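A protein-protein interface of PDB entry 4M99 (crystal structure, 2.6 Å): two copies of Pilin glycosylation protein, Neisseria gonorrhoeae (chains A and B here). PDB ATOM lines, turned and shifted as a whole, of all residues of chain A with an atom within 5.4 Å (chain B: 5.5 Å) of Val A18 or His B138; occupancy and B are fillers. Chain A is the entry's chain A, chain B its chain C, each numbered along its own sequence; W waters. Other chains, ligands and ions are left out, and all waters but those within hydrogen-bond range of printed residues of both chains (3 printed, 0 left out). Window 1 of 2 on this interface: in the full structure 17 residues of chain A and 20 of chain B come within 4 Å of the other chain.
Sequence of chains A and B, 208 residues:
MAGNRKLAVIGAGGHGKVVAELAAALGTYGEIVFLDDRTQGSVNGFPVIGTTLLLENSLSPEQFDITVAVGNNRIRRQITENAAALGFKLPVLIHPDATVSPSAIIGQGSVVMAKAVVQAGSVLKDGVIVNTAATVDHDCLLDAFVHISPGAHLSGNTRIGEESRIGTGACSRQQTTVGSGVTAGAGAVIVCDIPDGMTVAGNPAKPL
Gly A14 touches His B138 (CA to ND1, 3.5 Å).
Val A18 touches Gln B119.
His B138 touches Val A18 (CB to CG2, 3.8 Å).
Ala B120 touches Glu A21 (CB to OE1, 3.3 Å).
Water W3 lies within hydrogen-bond range of OE1 of Glu A21 (2.7 Å), OE1 of Gln B119 (2.7 Å) and N of Ala B120 (2.9 Å).
Water W1 bridges the side-chain carboxylate (OD1) of Asp B137 (2.7 Å) and the side-chain hydroxyl (OG1) of Thr A132 (3.4 Å).
Water W2 lies within hydrogen-bond range of NE2 of Gln B119 (2.9 Å) and SD of Met A113 (3.6 Å).
Of the 13 printed residues of chain A, 5 touch a printed residue of chain B.
Hydrophobic or aromatic side chains of chain A that line the printed part of chain B: Val A18.
Printed residues of chain B that touch a printed residue of chain A: Gln B119, Ala B120, Asp B137, His B138 and Asp B139.
Hydrophobic or aromatic side chains of chain B within 4 Å of the printed part of chain A: Ala B120 and His B138.
Among the printed residues, Asp or Glu carboxylates within 4 Å of a Lys or Arg side-chain nitrogen of the other chain: Lys A17 with Asp B139 (2.6 Å).
Of the printed residues of chain B, Gly A14 touches His B138.
Printed residues of chain B within 4 Å of Lys A17: Asp B139.
Val A18 touches two residues of chain B.
Of the printed residues of chain B, Glu A21 touches Ala B120.
Val B136 touches none of the printed residues of chain A.
Printed residues of chain A within 4 Å of Asp B137: Thr A132.
The nearest residue of chain B that does not touch Val A18 is Asp B137 (4.3 Å).
The nearest residue of chain A that does not touch His B138 is His A15 (4.04 Å).
The side-chain amino group of Lys A17 is in salt-bridge range of the side-chain carboxylate of Asp B139 (2.6 Å).
OD2 of Asp B137 is in hydrogen-bond range of OG1 of Thr A132 (2.7 Å).
The side-chain amide nitrogen (NE2) of Gln B119 is in hydrogen-bond range of the side-chain hydroxyl (OG1) of Thr A132, at 3.1 Å.
The backbone carbonyl oxygen (O) of Asp B137 sits at hydrogen-bond distance from the side-chain sulfur (SG) of Cys B140 (3.4 Å).
The backbone carbonyl oxygen (O) of His B138 is in hydrogen-bond range of the backbone NH (N) of Asn B157 (2.9 Å).
OD2 of Asp B139 lies within hydrogen-bond range of ND1 of His B138, at 2.9 Å.
The backbone carbonyl oxygen (O) of Ala B120 sits at hydrogen-bond distance from the backbone NH (N) of Asp B139 (3.0 Å).
The backbone carbonyl oxygen of Gln B119 lies close to the side-chain hydroxyl of Ser B122 (3.4 Å).
The backbone NH of Gln B119 is in hydrogen-bond range of the backbone carbonyl oxygen of Val B136 (2.9 Å).
No position is printed for both chains.
Of the 7 pairs that touch across the chains among the printed residues, none has its exchanged pair printed and touching as well.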
ATOM      1  N   GLY A  13       3.122   5.603 -15.625  1.00  0.00           N
ATOM      2  CA  GLY A  13       2.384   5.772 -16.861  1.00  0.00           C
ATOM      3  C   GLY A  13       2.571   4.604 -17.823  1.00  0.00           C
ATOM      4  O   GLY A  13       3.008   3.513 -17.435  1.00  0.00           O
ATOM      5  N   GLY A  14       2.234   4.829 -19.092  1.00  0.00           N
ATOM      6  CA  GLY A  14       2.294   3.786 -20.110  1.00  0.00           C
ATOM      7  C   GLY A  14       3.732   3.408 -20.423  1.00  0.00           C
ATOM      8  O   GLY A  14       4.061   2.221 -20.598  1.00  0.00           O
ATOM      9  N   HIS A  15       4.590   4.421 -20.489  1.00  0.00           N
ATOM     10  CA  HIS A  15       6.013   4.193 -20.586  1.00  0.00           C
ATOM     11  C   HIS A  15       6.499   3.341 -19.404  1.00  0.00           C
ATOM     12  O   HIS A  15       7.182   2.325 -19.600  1.00  0.00           O
ATOM     13  CB  HIS A  15       6.775   5.506 -20.613  1.00  0.00           C
ATOM     14  CG  HIS A  15       8.226   5.341 -20.931  1.00  0.00           C
ATOM     15  ND1 HIS A  15       9.229   5.822 -20.113  1.00  0.00           N
ATOM     16  CD2 HIS A  15       8.842   4.745 -21.975  1.00  0.00           C
ATOM     17  CE1 HIS A  15      10.401   5.531 -20.649  1.00  0.00           C
ATOM     18  NE2 HIS A  15      10.192   4.879 -21.779  1.00  0.00           N
ATOM     19  N   GLY A  16       6.139   3.754 -18.189  1.00  0.00           N
ATOM     20  CA  GLY A  16       6.473   2.991 -17.004  1.00  0.00           C
ATOM     21  C   GLY A  16       6.090   1.526 -17.106  1.00  0.00           C
ATOM     22  O   GLY A  16       6.808   0.648 -16.635  1.00  0.00           O
ATOM     23  N   LYS A  17       4.958   1.249 -17.736  1.00  0.00           N
ATOM     24  CA  LYS A  17       4.504  -0.125 -17.842  1.00  0.00           C
ATOM     25  C   LYS A  17       5.416  -0.928 -18.751  1.00  0.00           C
ATOM     26  O   LYS A  17       5.678  -2.091 -18.501  1.00  0.00           O
ATOM     27  CB  LYS A  17       3.066  -0.187 -18.356  1.00  0.00           C
ATOM     28  CG  LYS A  17       2.014  -0.031 -17.279  1.00  0.00           C
ATOM     29  CD  LYS A  17       0.685  -0.620 -17.743  1.00  0.00           C
ATOM     30  CE  LYS A  17       0.028   0.245 -18.812  1.00  0.00           C
ATOM     31  NZ  LYS A  17      -1.215  -0.389 -19.330  1.00  0.00           N
ATOM     32  N   VAL A  18       5.895  -0.301 -19.816  1.00  0.00           N
ATOM     33  CA  VAL A  18       6.771  -0.993 -20.748  1.00  0.00           C
ATOM     34  C   VAL A  18       8.158  -1.231 -20.141  1.00  0.00           C
ATOM     35  O   VAL A  18       8.738  -2.309 -20.315  1.00  0.00           O
ATOM     36  CB  VAL A  18       6.899  -0.233 -22.086  1.00  0.00           C
ATOM     37  CG1 VAL A  18       7.651  -1.087 -23.098  1.00  0.00           C
ATOM     38  CG2 VAL A  18       5.528   0.112 -22.624  1.00  0.00           C
ATOM     39  N   VAL A  19       8.681  -0.225 -19.434  1.00  0.00           N
ATOM     40  CA  VAL A  19       9.985  -0.334 -18.802  1.00  0.00           C
ATOM     41  C   VAL A  19       9.958  -1.393 -17.697  1.00  0.00           C
ATOM     42  O   VAL A  19      10.897  -2.171 -17.550  1.00  0.00           O
ATOM     43  CB  VAL A  19      10.431   0.996 -18.200  1.00  0.00           C
ATOM     44  CG1 VAL A  19      11.733   0.811 -17.388  1.00  0.00           C
ATOM     45  CG2 VAL A  19      10.606   2.039 -19.290  1.00  0.00           C
ATOM     46  N   ALA A  20       8.881  -1.420 -16.920  1.00  0.00           N
ATOM     47  CA  ALA A  20       8.769  -2.394 -15.849  1.00  0.00           C
ATOM     48  C   ALA A  20       8.748  -3.782 -16.448  1.00  0.00           C
ATOM     49  O   ALA A  20       9.385  -4.703 -15.931  1.00  0.00           O
ATOM     50  CB  ALA A  20       7.531  -2.154 -15.031  1.00  0.00           C
ATOM     51  N   GLU A  21       8.021  -3.934 -17.548  1.00  0.00           N
ATOM     52  CA  GLU A  21       8.006  -5.204 -18.258  1.00  0.00           C
ATOM     53  C   GLU A  21       9.364  -5.513 -18.904  1.00  0.00           C
ATOM     54  O   GLU A  21       9.760  -6.677 -18.998  1.00  0.00           O
ATOM     55  CB  GLU A  21       6.879  -5.248 -19.280  1.00  0.00           C
ATOM     56  CG  GLU A  21       5.539  -5.590 -18.658  1.00  0.00           C
ATOM     57  CD  GLU A  21       4.445  -5.861 -19.686  1.00  0.00           C
ATOM     58  OE1 GLU A  21       4.681  -5.673 -20.912  1.00  0.00           O
ATOM     59  OE2 GLU A  21       3.341  -6.270 -19.253  1.00  0.00           O
ATOM     60  N   LEU A  22      10.079  -4.477 -19.331  1.00  0.00           N
ATOM     61  CA  LEU A  22      11.419  -4.674 -19.857  1.00  0.00           C
ATOM     62  C   LEU A  22      12.265  -5.332 -18.786  1.00  0.00           C
ATOM     63  O   LEU A  22      12.891  -6.368 -19.026  1.00  0.00           O
ATOM     64  CB  LEU A  22      12.054  -3.344 -20.273  1.00  0.00           C
ATOM     65  CG  LEU A  22      13.401  -3.391 -21.004  1.00  0.00           C
ATOM     66  CD1 LEU A  22      13.599  -2.108 -21.785  1.00  0.00           C
ATOM     67  CD2 LEU A  22      14.584  -3.615 -20.062  1.00  0.00           C
ATOM     68  N   ALA A  23      12.285  -4.711 -17.607  1.00  0.00           N
ATOM     69  CA  ALA A  23      13.078  -5.190 -16.480  1.00  0.00           C
ATOM     70  C   ALA A  23      12.623  -6.565 -16.027  1.00  0.00           C
ATOM     71  O   ALA A  23      13.438  -7.396 -15.623  1.00  0.00           O
ATOM     72  CB  ALA A  23      12.994  -4.214 -15.341  1.00  0.00           C
ATOM     73  N   MET A 113      14.519  -0.477 -25.940  1.00  0.00           N
ATOM     74  CA  MET A 113      13.286  -1.261 -25.916  1.00  0.00           C
ATOM     75  C   MET A 113      13.327  -2.546 -26.749  1.00  0.00           C
ATOM     76  O   MET A 113      14.274  -2.781 -27.504  1.00  0.00           O
ATOM     77  CB  MET A 113      12.104  -0.368 -26.323  1.00  0.00           C
ATOM     78  CG  MET A 113      11.848   0.777 -25.323  1.00  0.00           C
ATOM     79  SD  MET A 113      11.294   0.176 -23.702  1.00  0.00           S
ATOM     80  CE  MET A 113      10.601   1.675 -22.996  1.00  0.00           C
ATOM     81  N   THR A 132      10.459   1.284 -28.899  1.00  0.00           N
ATOM     82  CA  THR A 132      10.135   0.035 -29.601  1.00  0.00           C
ATOM     83  C   THR A 132      10.605  -0.032 -31.064  1.00  0.00           C
ATOM     84  O   THR A 132      10.193   0.772 -31.893  1.00  0.00           O
ATOM     85  CB  THR A 132       8.629  -0.253 -29.561  1.00  0.00           C
ATOM     86  OG1 THR A 132       8.115   0.093 -28.269  1.00  0.00           O
ATOM     87  CG2 THR A 132       8.337  -1.742 -29.844  1.00  0.00           C
ATOM     88  N   GLN B 119       3.195  -4.246 -27.262  1.00  0.00           N
ATOM     89  CA  GLN B 119       3.536  -3.808 -25.905  1.00  0.00           C
ATOM     90  C   GLN B 119       2.380  -3.891 -24.891  1.00  0.00           C
ATOM     91  O   GLN B 119       1.257  -4.291 -25.226  1.00  0.00           O
ATOM     92  CB  GLN B 119       4.130  -2.399 -25.933  1.00  0.00           C
ATOM     93  CG  GLN B 119       5.410  -2.273 -26.762  1.00  0.00           C
ATOM     94  CD  GLN B 119       6.648  -2.859 -26.062  1.00  0.00           C
ATOM     95  OE1 GLN B 119       6.554  -3.817 -25.283  1.00  0.00           O
ATOM     96  NE2 GLN B 119       7.817  -2.285 -26.350  1.00  0.00           N
ATOM     97  N   ALA B 120       2.682  -3.511 -23.649  1.00  0.00           N
ATOM     98  CA  ALA B 120       1.817  -3.753 -22.480  1.00  0.00           C
ATOM     99  C   ALA B 120       0.405  -3.166 -22.553  1.00  0.00           C
ATOM    100  O   ALA B 120       0.212  -2.002 -22.965  1.00  0.00           O
ATOM    101  CB  ALA B 120       2.504  -3.250 -21.221  1.00  0.00           C
ATOM    102  N   GLY B 121      -0.571  -3.967 -22.129  1.00  0.00           N
ATOM    103  CA  GLY B 121      -1.944  -3.509 -22.030  1.00  0.00           C
ATOM    104  C   GLY B 121      -2.663  -3.358 -23.360  1.00  0.00           C
ATOM    105  O   GLY B 121      -3.849  -3.012 -23.402  1.00  0.00           O
ATOM    106  N   SER B 122      -1.948  -3.600 -24.455  1.00  0.00           N
ATOM    107  CA  SER B 122      -2.575  -3.620 -25.761  1.00  0.00           C
ATOM    108  C   SER B 122      -3.635  -4.702 -25.823  1.00  0.00           C
ATOM    109  O   SER B 122      -3.441  -5.830 -25.340  1.00  0.00           O
ATOM    110  CB  SER B 122      -1.540  -3.831 -26.860  1.00  0.00           C
ATOM    111  OG  SER B 122      -0.931  -2.600 -27.210  1.00  0.00           O
ATOM    112  N   VAL B 136       2.953  -2.473 -32.283  1.00  0.00           N
ATOM    113  CA  VAL B 136       1.756  -1.954 -31.667  1.00  0.00           C
ATOM    114  C   VAL B 136       2.146  -1.608 -30.243  1.00  0.00           C
ATOM    115  O   VAL B 136       2.322  -2.497 -29.401  1.00  0.00           O
ATOM    116  CB  VAL B 136       0.678  -3.044 -31.649  1.00  0.00           C
ATOM    117  CG1 VAL B 136      -0.566  -2.579 -30.893  1.00  0.00           C
ATOM    118  CG2 VAL B 136       0.338  -3.458 -33.073  1.00  0.00           C
ATOM    119  N   ASP B 137       2.326  -0.325 -29.962  1.00  0.00           N
ATOM    120  CA  ASP B 137       2.802   0.024 -28.639  1.00  0.00           C
ATOM    121  C   ASP B 137       1.771  -0.090 -27.524  1.00  0.00           C
ATOM    122  O   ASP B 137       0.739  -0.755 -27.678  1.00  0.00           O
ATOM    123  CB  ASP B 137       3.491   1.368 -28.623  1.00  0.00           C
ATOM    124  CG  ASP B 137       4.864   1.272 -28.010  1.00  0.00           C
ATOM    125  OD1 ASP B 137       4.931   0.985 -26.794  1.00  0.00           O
ATOM    126  OD2 ASP B 137       5.866   1.434 -28.748  1.00  0.00           O
ATOM    127  N   HIS B 138       2.069   0.544 -26.393  1.00  0.00           N
ATOM    128  CA  HIS B 138       1.305   0.307 -25.169  1.00  0.00           C
ATOM    129  C   HIS B 138      -0.127   0.838 -25.224  1.00  0.00           C
ATOM    130  O   HIS B 138      -0.371   1.944 -25.709  1.00  0.00           O
ATOM    131  CB  HIS B 138       2.053   0.856 -23.945  1.00  0.00           C
ATOM    132  CG  HIS B 138       2.209   2.345 -23.939  1.00  0.00           C
ATOM    133  ND1 HIS B 138       1.282   3.190 -23.358  1.00  0.00           N
ATOM    134  CD2 HIS B 138       3.191   3.141 -24.424  1.00  0.00           C
ATOM    135  CE1 HIS B 138       1.689   4.440 -23.491  1.00  0.00           C
ATOM    136  NE2 HIS B 138       2.843   4.441 -24.134  1.00  0.00           N
ATOM    137  N   ASP B 139      -1.060   0.027 -24.726  1.00  0.00           N
ATOM    138  CA  ASP B 139      -2.456   0.430 -24.564  1.00  0.00           C
ATOM    139  C   ASP B 139      -3.122   0.775 -25.889  1.00  0.00           C
ATOM    140  O   ASP B 139      -3.929   1.695 -25.972  1.00  0.00           O
ATOM    141  CB  ASP B 139      -2.565   1.619 -23.617  1.00  0.00           C
ATOM    142  CG  ASP B 139      -1.927   1.344 -22.274  1.00  0.00           C
ATOM    143  OD1 ASP B 139      -2.347   0.368 -21.596  1.00  0.00           O
ATOM    144  OD2 ASP B 139      -0.993   2.104 -21.919  1.00  0.00           O
ATOM    145  N   CYS B 140      -2.767   0.039 -26.929  1.00  0.00           N
ATOM    146  CA  CYS B 140      -3.442   0.192 -28.190  1.00  0.00           C
ATOM    147  C   CYS B 140      -4.629  -0.763 -28.240  1.00  0.00           C
ATOM    148  O   CYS B 140      -4.626  -1.821 -27.600  1.00  0.00           O
ATOM    149  CB  CYS B 140      -2.489  -0.061 -29.354  1.00  0.00           C
ATOM    150  SG  CYS B 140      -1.270   1.238 -29.577  1.00  0.00           S
ATOM    151  N   SER B 155       1.881   4.301 -32.285  1.00  0.00           N
ATOM    152  CA  SER B 155       2.259   4.854 -30.988  1.00  0.00           C
ATOM    153  C   SER B 155       1.302   4.397 -29.897  1.00  0.00           C
ATOM    154  O   SER B 155       0.371   3.619 -30.158  1.00  0.00           O
ATOM    155  CB  SER B 155       2.344   6.369 -31.037  1.00  0.00           C
ATOM    156  OG  SER B 155       3.326   6.783 -31.967  1.00  0.00           O
ATOM    157  N   GLY B 156       1.541   4.857 -28.670  1.00  0.00           N
ATOM    158  CA  GLY B 156       0.721   4.434 -27.543  1.00  0.00           C
ATOM    159  C   GLY B 156      -0.712   4.957 -27.639  1.00  0.00           C
ATOM    160  O   GLY B 156      -0.942   6.043 -28.172  1.00  0.00           O
ATOM    161  N   ASN B 157      -1.662   4.192 -27.107  1.00  0.00           N
ATOM    162  CA  ASN B 157      -3.076   4.545 -27.146  1.00  0.00           C
ATOM    163  C   ASN B 157      -3.532   4.876 -28.560  1.00  0.00           C
ATOM    164  O   ASN B 157      -4.061   5.959 -28.827  1.00  0.00           O
ATOM    165  CB  ASN B 157      -3.380   5.704 -26.193  1.00  0.00           C
ATOM    166  CG  ASN B 157      -3.101   5.355 -24.741  1.00  0.00           C
ATOM    167  OD1 ASN B 157      -3.870   4.631 -24.103  1.00  0.00           O
ATOM    168  ND2 ASN B 157      -1.999   5.870 -24.214  1.00  0.00           N
ATOM    169  N   THR B 158      -3.288   3.942 -29.470  1.00  0.00           N
ATOM    170  CA  THR B 158      -3.859   4.015 -30.797  1.00  0.00           C
ATOM    171  C   THR B 158      -5.029   3.042 -30.858  1.00  0.00           C
ATOM    172  O   THR B 158      -4.925   1.903 -30.375  1.00  0.00           O
ATOM    173  CB  THR B 158      -2.820   3.675 -31.864  1.00  0.00           C
ATOM    174  OG1 THR B 158      -1.844   4.723 -31.922  1.00  0.00           O
ATOM    175  CG2 THR B 158      -3.474   3.529 -33.226  1.00  0.00           C
HETATM  176  O   HOH W   1       7.136   1.972 -25.605  1.00  0.00           O
HETATM  177  O   HOH W   2       9.993  -3.067 -24.597  1.00  0.00           O
HETATM  178  O   HOH W   3       5.450  -3.975 -22.833  1.00  0.00           O
